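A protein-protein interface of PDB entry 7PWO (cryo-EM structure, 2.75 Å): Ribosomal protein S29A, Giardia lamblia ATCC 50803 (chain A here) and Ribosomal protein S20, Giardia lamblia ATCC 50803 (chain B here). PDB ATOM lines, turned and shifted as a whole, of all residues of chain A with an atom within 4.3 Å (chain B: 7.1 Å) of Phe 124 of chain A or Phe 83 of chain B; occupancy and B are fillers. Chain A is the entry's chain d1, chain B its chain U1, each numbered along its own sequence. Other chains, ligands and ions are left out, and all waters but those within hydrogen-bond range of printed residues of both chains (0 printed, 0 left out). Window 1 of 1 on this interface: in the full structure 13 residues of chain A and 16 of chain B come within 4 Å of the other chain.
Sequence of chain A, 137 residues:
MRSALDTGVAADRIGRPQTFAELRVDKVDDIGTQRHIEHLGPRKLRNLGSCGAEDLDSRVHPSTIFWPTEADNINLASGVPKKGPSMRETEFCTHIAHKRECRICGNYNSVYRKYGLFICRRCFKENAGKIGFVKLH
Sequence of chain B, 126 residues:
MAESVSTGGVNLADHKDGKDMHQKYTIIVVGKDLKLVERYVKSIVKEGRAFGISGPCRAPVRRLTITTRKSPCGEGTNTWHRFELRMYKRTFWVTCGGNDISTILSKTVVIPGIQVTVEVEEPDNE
Of the printed residues of chain B, Arg 121 of chain A touches Thr 68.
Arg 122 of chain A touches none of the printed residues of chain B.
Of chain B, only Ile 66 (3.4 Å) and Phe 83 (3.3 Å) come within 4 Å of Phe 124 of chain A.
Of the printed residues of chain B, Phe 133 of chain A touches Leu 64, Ile 66, Phe 83, Glu 84 and Leu 85.
Thr 67 of chain B touches none of the printed residues of chain A.
Of the printed residues of chain A, Arg 82 of chain B touches Lys 135.
Phe 83 of chain B touches four residues of chain A.
The nearest printed residue of chain A that does not touch Leu 85 of chain B is Val 134 of chain A (5.4 Å).
Of the 11 printed residues of chain B, 8 touch a printed residue of chain A.
Of the 13 printed residues of chain A, 6 touch a printed residue of chain B.
Among the printed residues, 15 pairs touch across the chains.
Among the printed residues, no Asp or Glu carboxylate lies within 4 Å of a Lys or Arg side-chain nitrogen of the other chain.
Thr 68 of chain B touches Arg 121 of chain A (OG1 to CB, 3.2 Å).
Phe 124 of chain A touches Ile 66 of chain B (CZ to CD1, 3.4 Å).
CE2 of Phe 124 of chain A touches CD2 of Phe 83 of chain B, at 3.3 Å.
Phe 83 of chain B touches Phe 133 of chain A.
Glu 84 of chain B touches Phe 133 of chain A.
Leu 85 of chain B touches Phe 133 of chain A (CD1 to N, 3.8 Å).
Val 134 of chain A touches Phe 83 of chain B.
NZ of Lys 135 of chain A touches CD2 of His 81 of chain B, at 3.0 Å.
NZ of Lys 135 of chain A touches N of Arg 82 of chain B (3.7 Å).
Lys 135 of chain A touches Phe 83 of chain B (CG to CE1, 3.9 Å).
The backbone NH (N) of Glu 84 of chain B lies within hydrogen-bond range of the backbone carbonyl oxygen (O) of Val 134 of chain A (3.2 Å).
NZ of Lys 125 of chain A lies close to ND1 of His 81 of chain B (3.2 Å).
O of Thr 68 of chain B is in hydrogen-bond range of NZ of Lys 125 of chain A, at 3.0 Å.
N of Phe 83 of chain B sits at hydrogen-bond distance from O of Ile 66 of chain B (2.8 Å).
N of Phe 133 of chain A is in hydrogen-bond range of O of Ala 128 of chain A, 2.9 Å away.
N of His 81 of chain B sits at hydrogen-bond distance from O of Thr 68 of chain B, at 2.9 Å.
The guanidinium group (NE) of Arg 63 of chain B is in salt-bridge range of the side-chain carboxylate (OE2) of Glu 84 of chain B (2.9 Å).
The backbone NH of Leu 64 of chain B sits at hydrogen-bond distance from the backbone carbonyl oxygen of Leu 85 of chain B (2.6 Å).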
ATOM      1  N   ILE A 119      21.141  11.099  -0.215  1.00  0.00           N
ATOM      2  CA  ILE A 119      22.588  10.853   0.066  1.00  0.00           C
ATOM      3  C   ILE A 119      23.218  10.307  -1.214  1.00  0.00           C
ATOM      4  O   ILE A 119      22.466  10.034  -2.161  1.00  0.00           O
ATOM      5  CB  ILE A 119      22.765   9.877   1.246  1.00  0.00           C
ATOM      6  CG1 ILE A 119      21.643   8.836   1.291  1.00  0.00           C
ATOM      7  CG2 ILE A 119      22.881  10.630   2.561  1.00  0.00           C
ATOM      8  CD1 ILE A 119      21.709   7.912   2.483  1.00  0.00           C
ATOM      9  N   CYS A 120      24.542  10.147  -1.235  1.00  0.00           N
ATOM     10  CA  CYS A 120      25.214   9.694  -2.482  1.00  0.00           C
ATOM     11  C   CYS A 120      25.659   8.234  -2.340  1.00  0.00           C
ATOM     12  O   CYS A 120      25.772   7.757  -1.193  1.00  0.00           O
ATOM     13  CB  CYS A 120      26.407  10.583  -2.822  1.00  0.00           C
ATOM     14  SG  CYS A 120      27.594  10.754  -1.467  1.00  0.00           S
ATOM     15  N   ARG A 121      25.927   7.567  -3.465  1.00  0.00           N
ATOM     16  CA  ARG A 121      26.303   6.128  -3.445  1.00  0.00           C
ATOM     17  C   ARG A 121      27.622   5.923  -2.698  1.00  0.00           C
ATOM     18  O   ARG A 121      27.708   4.960  -1.910  1.00  0.00           O
ATOM     19  CB  ARG A 121      26.405   5.593  -4.876  1.00  0.00           C
ATOM     20  N   ARG A 122      28.614   6.768  -2.969  1.00  0.00           N
ATOM     21  CA  ARG A 122      29.902   6.685  -2.237  1.00  0.00           C
ATOM     22  C   ARG A 122      29.633   6.768  -0.729  1.00  0.00           C
ATOM     23  O   ARG A 122      30.059   5.848  -0.011  1.00  0.00           O
ATOM     24  CB  ARG A 122      30.843   7.786  -2.734  1.00  0.00           C
ATOM     25  CG  ARG A 122      31.226   7.633  -4.198  1.00  0.00           C
ATOM     26  CD  ARG A 122      31.788   8.884  -4.840  1.00  0.00           C
ATOM     27  NE  ARG A 122      32.197   8.590  -6.205  1.00  0.00           N
ATOM     28  CZ  ARG A 122      32.615   9.494  -7.082  1.00  0.00           C
ATOM     29  NH1 ARG A 122      32.678  10.768  -6.742  1.00  0.00           N
ATOM     30  NH2 ARG A 122      32.962   9.119  -8.299  1.00  0.00           N
ATOM     31  N   CYS A 123      28.943   7.818  -0.277  1.00  0.00           N
ATOM     32  CA  CYS A 123      28.642   7.986   1.173  1.00  0.00           C
ATOM     33  C   CYS A 123      27.791   6.814   1.648  1.00  0.00           C
ATOM     34  O   CYS A 123      27.972   6.387   2.803  1.00  0.00           O
ATOM     35  CB  CYS A 123      27.881   9.278   1.439  1.00  0.00           C
ATOM     36  SG  CYS A 123      28.919  10.602   2.113  1.00  0.00           S
ATOM     37  N   PHE A 124      26.916   6.308   0.778  1.00  0.00           N
ATOM     38  CA  PHE A 124      25.983   5.217   1.166  1.00  0.00           C
ATOM     39  C   PHE A 124      26.749   3.992   1.668  1.00  0.00           C
ATOM     40  O   PHE A 124      26.329   3.431   2.685  1.00  0.00           O
ATOM     41  CB  PHE A 124      25.081   4.853  -0.017  1.00  0.00           C
ATOM     42  CG  PHE A 124      24.015   3.828   0.275  1.00  0.00           C
ATOM     43  CD1 PHE A 124      22.897   4.159   1.025  1.00  0.00           C
ATOM     44  CD2 PHE A 124      24.122   2.535  -0.211  1.00  0.00           C
ATOM     45  CE1 PHE A 124      21.915   3.217   1.288  1.00  0.00           C
ATOM     46  CE2 PHE A 124      23.139   1.595   0.052  1.00  0.00           C
ATOM     47  CZ  PHE A 124      22.038   1.938   0.800  1.00  0.00           C
ATOM     48  N   LYS A 125      27.842   3.615   1.013  1.00  0.00           N
ATOM     49  CA  LYS A 125      28.545   2.352   1.374  1.00  0.00           C
ATOM     50  C   LYS A 125      29.037   2.347   2.828  1.00  0.00           C
ATOM     51  O   LYS A 125      28.810   1.326   3.505  1.00  0.00           O
ATOM     52  CB  LYS A 125      29.732   2.135   0.432  1.00  0.00           C
ATOM     53  CG  LYS A 125      29.415   2.260  -1.051  1.00  0.00           C
ATOM     54  CD  LYS A 125      28.770   1.027  -1.642  1.00  0.00           C
ATOM     55  CE  LYS A 125      28.492   1.169  -3.123  1.00  0.00           C
ATOM     56  NZ  LYS A 125      28.173  -0.133  -3.754  1.00  0.00           N
ATOM     57  N   GLU A 126      29.679   3.423   3.295  1.00  0.00           N
ATOM     58  CA  GLU A 126      30.301   3.416   4.652  1.00  0.00           C
ATOM     59  C   GLU A 126      29.306   3.770   5.769  1.00  0.00           C
ATOM     60  O   GLU A 126      29.724   3.725   6.938  1.00  0.00           O
ATOM     61  CB  GLU A 126      31.490   4.379   4.684  1.00  0.00           C
ATOM     62  CG  GLU A 126      31.160   5.776   4.195  1.00  0.00           C
ATOM     63  CD  GLU A 126      31.328   5.953   2.697  1.00  0.00           C
ATOM     64  OE1 GLU A 126      31.397   7.111   2.240  1.00  0.00           O
ATOM     65  OE2 GLU A 126      31.391   4.929   1.991  1.00  0.00           O
ATOM     66  N   ASN A 127      28.061   4.121   5.443  1.00  0.00           N
ATOM     67  CA  ASN A 127      27.060   4.431   6.449  1.00  0.00           C
ATOM     68  C   ASN A 127      25.770   3.666   6.249  1.00  0.00           C
ATOM     69  O   ASN A 127      24.887   3.761   7.102  1.00  0.00           O
ATOM     70  CB  ASN A 127      26.759   5.937   6.488  1.00  0.00           C
ATOM     71  CG  ASN A 127      27.962   6.759   6.904  1.00  0.00           C
ATOM     72  OD1 ASN A 127      28.486   7.546   6.130  1.00  0.00           O
ATOM     73  ND2 ASN A 127      28.417   6.558   8.138  1.00  0.00           N
ATOM     74  N   ALA A 128      25.624   2.922   5.154  1.00  0.00           N
ATOM     75  CA  ALA A 128      24.426   2.114   4.978  1.00  0.00           C
ATOM     76  C   ALA A 128      24.400   0.957   5.964  1.00  0.00           C
ATOM     77  O   ALA A 128      23.322   0.513   6.377  1.00  0.00           O
ATOM     78  CB  ALA A 128      24.343   1.609   3.540  1.00  0.00           C
ATOM     79  N   PHE A 133      21.000  -1.046   5.580  1.00  0.00           N
ATOM     80  CA  PHE A 133      21.175  -1.820   4.362  1.00  0.00           C
ATOM     81  C   PHE A 133      22.285  -2.848   4.545  1.00  0.00           C
ATOM     82  O   PHE A 133      23.396  -2.520   4.967  1.00  0.00           O
ATOM     83  CB  PHE A 133      21.465  -0.879   3.200  1.00  0.00           C
ATOM     84  CG  PHE A 133      20.303   0.001   2.849  1.00  0.00           C
ATOM     85  CD1 PHE A 133      19.269  -0.472   2.064  1.00  0.00           C
ATOM     86  CD2 PHE A 133      20.191   1.263   3.399  1.00  0.00           C
ATOM     87  CE1 PHE A 133      18.182   0.326   1.768  1.00  0.00           C
ATOM     88  CE2 PHE A 133      19.103   2.068   3.106  1.00  0.00           C
ATOM     89  CZ  PHE A 133      18.099   1.596   2.289  1.00  0.00           C
ATOM     90  N   VAL A 134      21.957  -4.106   4.248  1.00  0.00           N
ATOM     91  CA  VAL A 134      22.830  -5.247   4.460  1.00  0.00           C
ATOM     92  C   VAL A 134      22.891  -6.046   3.166  1.00  0.00           C
ATOM     93  O   VAL A 134      22.179  -5.766   2.203  1.00  0.00           O
ATOM     94  CB  VAL A 134      22.357  -6.135   5.636  1.00  0.00           C
ATOM     95  CG1 VAL A 134      22.519  -5.407   6.942  1.00  0.00           C
ATOM     96  CG2 VAL A 134      20.908  -6.531   5.442  1.00  0.00           C
ATOM     97  N   LYS A 135      23.766  -7.048   3.155  1.00  0.00           N
ATOM     98  CA  LYS A 135      24.053  -7.844   1.967  1.00  0.00           C
ATOM     99  C   LYS A 135      23.737  -9.310   2.212  1.00  0.00           C
ATOM    100  O   LYS A 135      24.210  -9.892   3.193  1.00  0.00           O
ATOM    101  CB  LYS A 135      25.516  -7.690   1.553  1.00  0.00           C
ATOM    102  CG  LYS A 135      25.846  -6.320   1.032  1.00  0.00           C
ATOM    103  CD  LYS A 135      27.309  -6.214   0.704  1.00  0.00           C
ATOM    104  CE  LYS A 135      27.571  -7.073  -0.514  1.00  0.00           C
ATOM    105  NZ  LYS A 135      26.907  -6.521  -1.715  1.00  0.00           N
ATOM    106  N   ARG B  63      10.311  -4.603   1.253  1.00  0.00           N
ATOM    107  CA  ARG B  63      11.759  -4.501   1.327  1.00  0.00           C
ATOM    108  C   ARG B  63      12.257  -3.242   0.637  1.00  0.00           C
ATOM    109  O   ARG B  63      11.683  -2.787  -0.358  1.00  0.00           O
ATOM    110  CB  ARG B  63      12.365  -5.795   0.752  1.00  0.00           C
ATOM    111  CG  ARG B  63      11.906  -6.105  -0.651  1.00  0.00           C
ATOM    112  CD  ARG B  63      12.256  -7.550  -1.057  1.00  0.00           C
ATOM    113  NE  ARG B  63      13.672  -7.811  -1.285  1.00  0.00           N
ATOM    114  CZ  ARG B  63      14.402  -7.181  -2.202  1.00  0.00           C
ATOM    115  NH1 ARG B  63      13.844  -6.272  -2.993  1.00  0.00           N
ATOM    116  NH2 ARG B  63      15.685  -7.478  -2.348  1.00  0.00           N
ATOM    117  N   LEU B  64      13.320  -2.678   1.194  1.00  0.00           N
ATOM    118  CA  LEU B  64      13.810  -1.351   0.853  1.00  0.00           C
ATOM    119  C   LEU B  64      15.196  -1.588   0.252  1.00  0.00           C
ATOM    120  O   LEU B  64      16.136  -1.913   0.989  1.00  0.00           O
ATOM    121  CB  LEU B  64      13.896  -0.505   2.126  1.00  0.00           C
ATOM    122  CG  LEU B  64      12.707   0.225   2.794  1.00  0.00           C
ATOM    123  CD1 LEU B  64      12.029   1.322   2.011  1.00  0.00           C
ATOM    124  CD2 LEU B  64      11.682  -0.780   3.297  1.00  0.00           C
ATOM    125  N   THR B  65      15.341  -1.470  -1.073  1.00  0.00           N
ATOM    126  CA  THR B  65      16.549  -2.005  -1.702  1.00  0.00           C
ATOM    127  C   THR B  65      17.158  -1.055  -2.725  1.00  0.00           C
ATOM    128  O   THR B  65      16.473  -0.214  -3.309  1.00  0.00           O
ATOM    129  CB  THR B  65      16.289  -3.353  -2.382  1.00  0.00           C
ATOM    130  OG1 THR B  65      15.265  -3.215  -3.374  1.00  0.00           O
ATOM    131  CG2 THR B  65      15.862  -4.370  -1.359  1.00  0.00           C
ATOM    132  N   ILE B  66      18.468  -1.219  -2.932  1.00  0.00           N
ATOM    133  CA  ILE B  66      19.262  -0.365  -3.810  1.00  0.00           C
ATOM    134  C   ILE B  66      20.358  -1.213  -4.445  1.00  0.00           C
ATOM    135  O   ILE B  66      20.846  -2.172  -3.845  1.00  0.00           O
ATOM    136  CB  ILE B  66      19.896   0.810  -3.031  1.00  0.00           C
ATOM    137  CG1 ILE B  66      18.856   1.551  -2.195  1.00  0.00           C
ATOM    138  CG2 ILE B  66      20.535   1.794  -3.983  1.00  0.00           C
ATOM    139  CD1 ILE B  66      19.466   2.552  -1.303  1.00  0.00           C
ATOM    140  N   THR B  67      20.755  -0.854  -5.665  1.00  0.00           N
ATOM    141  CA  THR B  67      21.970  -1.381  -6.268  1.00  0.00           C
ATOM    142  C   THR B  67      22.850  -0.214  -6.680  1.00  0.00           C
ATOM    143  O   THR B  67      22.360   0.874  -6.993  1.00  0.00           O
ATOM    144  CB  THR B  67      21.693  -2.292  -7.467  1.00  0.00           C
ATOM    145  OG1 THR B  67      21.019  -1.557  -8.491  1.00  0.00           O
ATOM    146  CG2 THR B  67      20.835  -3.472  -7.049  1.00  0.00           C
ATOM    147  N   THR B  68      24.159  -0.447  -6.665  1.00  0.00           N
ATOM    148  CA  THR B  68      25.122   0.642  -6.643  1.00  0.00           C
ATOM    149  C   THR B  68      26.520   0.090  -6.904  1.00  0.00           C
ATOM    150  O   THR B  68      26.886  -0.955  -6.366  1.00  0.00           O
ATOM    151  CB  THR B  68      25.028   1.394  -5.294  1.00  0.00           C
ATOM    152  OG1 THR B  68      25.987   2.454  -5.232  1.00  0.00           O
ATOM    153  CG2 THR B  68      25.132   0.451  -4.076  1.00  0.00           C
ATOM    154  N   HIS B  81      27.230  -3.733  -5.802  1.00  0.00           N
ATOM    155  CA  HIS B  81      26.633  -4.042  -4.515  1.00  0.00           C
ATOM    156  C   HIS B  81      25.119  -3.965  -4.610  1.00  0.00           C
ATOM    157  O   HIS B  81      24.566  -3.046  -5.218  1.00  0.00           O
ATOM    158  CB  HIS B  81      27.134  -3.083  -3.446  1.00  0.00           C
ATOM    159  CG  HIS B  81      28.425  -3.492  -2.822  1.00  0.00           C
ATOM    160  ND1 HIS B  81      29.168  -2.644  -2.031  1.00  0.00           N
ATOM    161  CD2 HIS B  81      29.059  -4.686  -2.791  1.00  0.00           C
ATOM    162  CE1 HIS B  81      30.233  -3.281  -1.586  1.00  0.00           C
ATOM    163  NE2 HIS B  81      30.186  -4.525  -2.025  1.00  0.00           N
ATOM    164  N   ARG B  82      24.453  -4.942  -4.010  1.00  0.00           N
ATOM    165  CA  ARG B  82      22.996  -4.984  -3.955  1.00  0.00           C
ATOM    166  C   ARG B  82      22.587  -4.966  -2.485  1.00  0.00           C
ATOM    167  O   ARG B  82      22.633  -5.999  -1.815  1.00  0.00           O
ATOM    168  CB  ARG B  82      22.456  -6.225  -4.654  1.00  0.00           C
ATOM    169  CG  ARG B  82      22.774  -6.322  -6.126  1.00  0.00           C
ATOM    170  CD  ARG B  82      22.613  -7.758  -6.615  1.00  0.00           C
ATOM    171  NE  ARG B  82      23.820  -8.564  -6.477  1.00  0.00           N
ATOM    172  CZ  ARG B  82      24.135  -9.564  -7.291  1.00  0.00           C
ATOM    173  NH1 ARG B  82      23.323  -9.892  -8.284  1.00  0.00           N
ATOM    174  NH2 ARG B  82      25.250 -10.250  -7.103  1.00  0.00           N
ATOM    175  N   PHE B  83      22.182  -3.800  -1.988  1.00  0.00           N
ATOM    176  CA  PHE B  83      21.724  -3.656  -0.612  1.00  0.00           C
ATOM    177  C   PHE B  83      20.221  -3.889  -0.511  1.00  0.00           C
ATOM    178  O   PHE B  83      19.469  -3.626  -1.451  1.00  0.00           O
ATOM    179  CB  PHE B  83      22.080  -2.274  -0.074  1.00  0.00           C
ATOM    180  CG  PHE B  83      23.534  -2.102   0.199  1.00  0.00           C
ATOM    181  CD1 PHE B  83      24.110  -2.657   1.327  1.00  0.00           C
ATOM    182  CD2 PHE B  83      24.342  -1.422  -0.702  1.00  0.00           C
ATOM    183  CE1 PHE B  83      25.450  -2.515   1.565  1.00  0.00           C
ATOM    184  CE2 PHE B  83      25.684  -1.270  -0.462  1.00  0.00           C
ATOM    185  CZ  PHE B  83      26.241  -1.818   0.668  1.00  0.00           C
ATOM    186  N   GLU B  84      19.792  -4.366   0.657  1.00  0.00           N
ATOM    187  CA  GLU B  84      18.449  -4.887   0.879  1.00  0.00           C
ATOM    188  C   GLU B  84      18.047  -4.696   2.333  1.00  0.00           C
ATOM    189  O   GLU B  84      18.895  -4.727   3.229  1.00  0.00           O
ATOM    190  CB  GLU B  84      18.371  -6.373   0.509  1.00  0.00           C
ATOM    191  CG  GLU B  84      16.998  -6.987   0.642  1.00  0.00           C
ATOM    192  CD  GLU B  84      16.957  -8.427   0.219  1.00  0.00           C
ATOM    193  OE1 GLU B  84      18.013  -8.975  -0.169  1.00  0.00           O
ATOM    194  OE2 GLU B  84      15.860  -9.014   0.267  1.00  0.00           O
ATOM    195  N   LEU B  85      16.747  -4.497   2.564  1.00  0.00           N
ATOM    196  CA  LEU B  85      16.258  -4.211   3.913  1.00  0.00           C
ATOM    197  C   LEU B  85      14.769  -4.536   3.992  1.00  0.00           C
ATOM    198  O   LEU B  85      13.954  -3.808   3.426  1.00  0.00           O
ATOM    199  CB  LEU B  85      16.537  -2.755   4.273  1.00  0.00           C
ATOM    200  CG  LEU B  85      16.128  -2.189   5.632  1.00  0.00           C
ATOM    201  CD1 LEU B  85      17.198  -1.265   6.136  1.00  0.00           C
ATOM    202  CD2 LEU B  85      14.828  -1.413   5.520  1.00  0.00           C
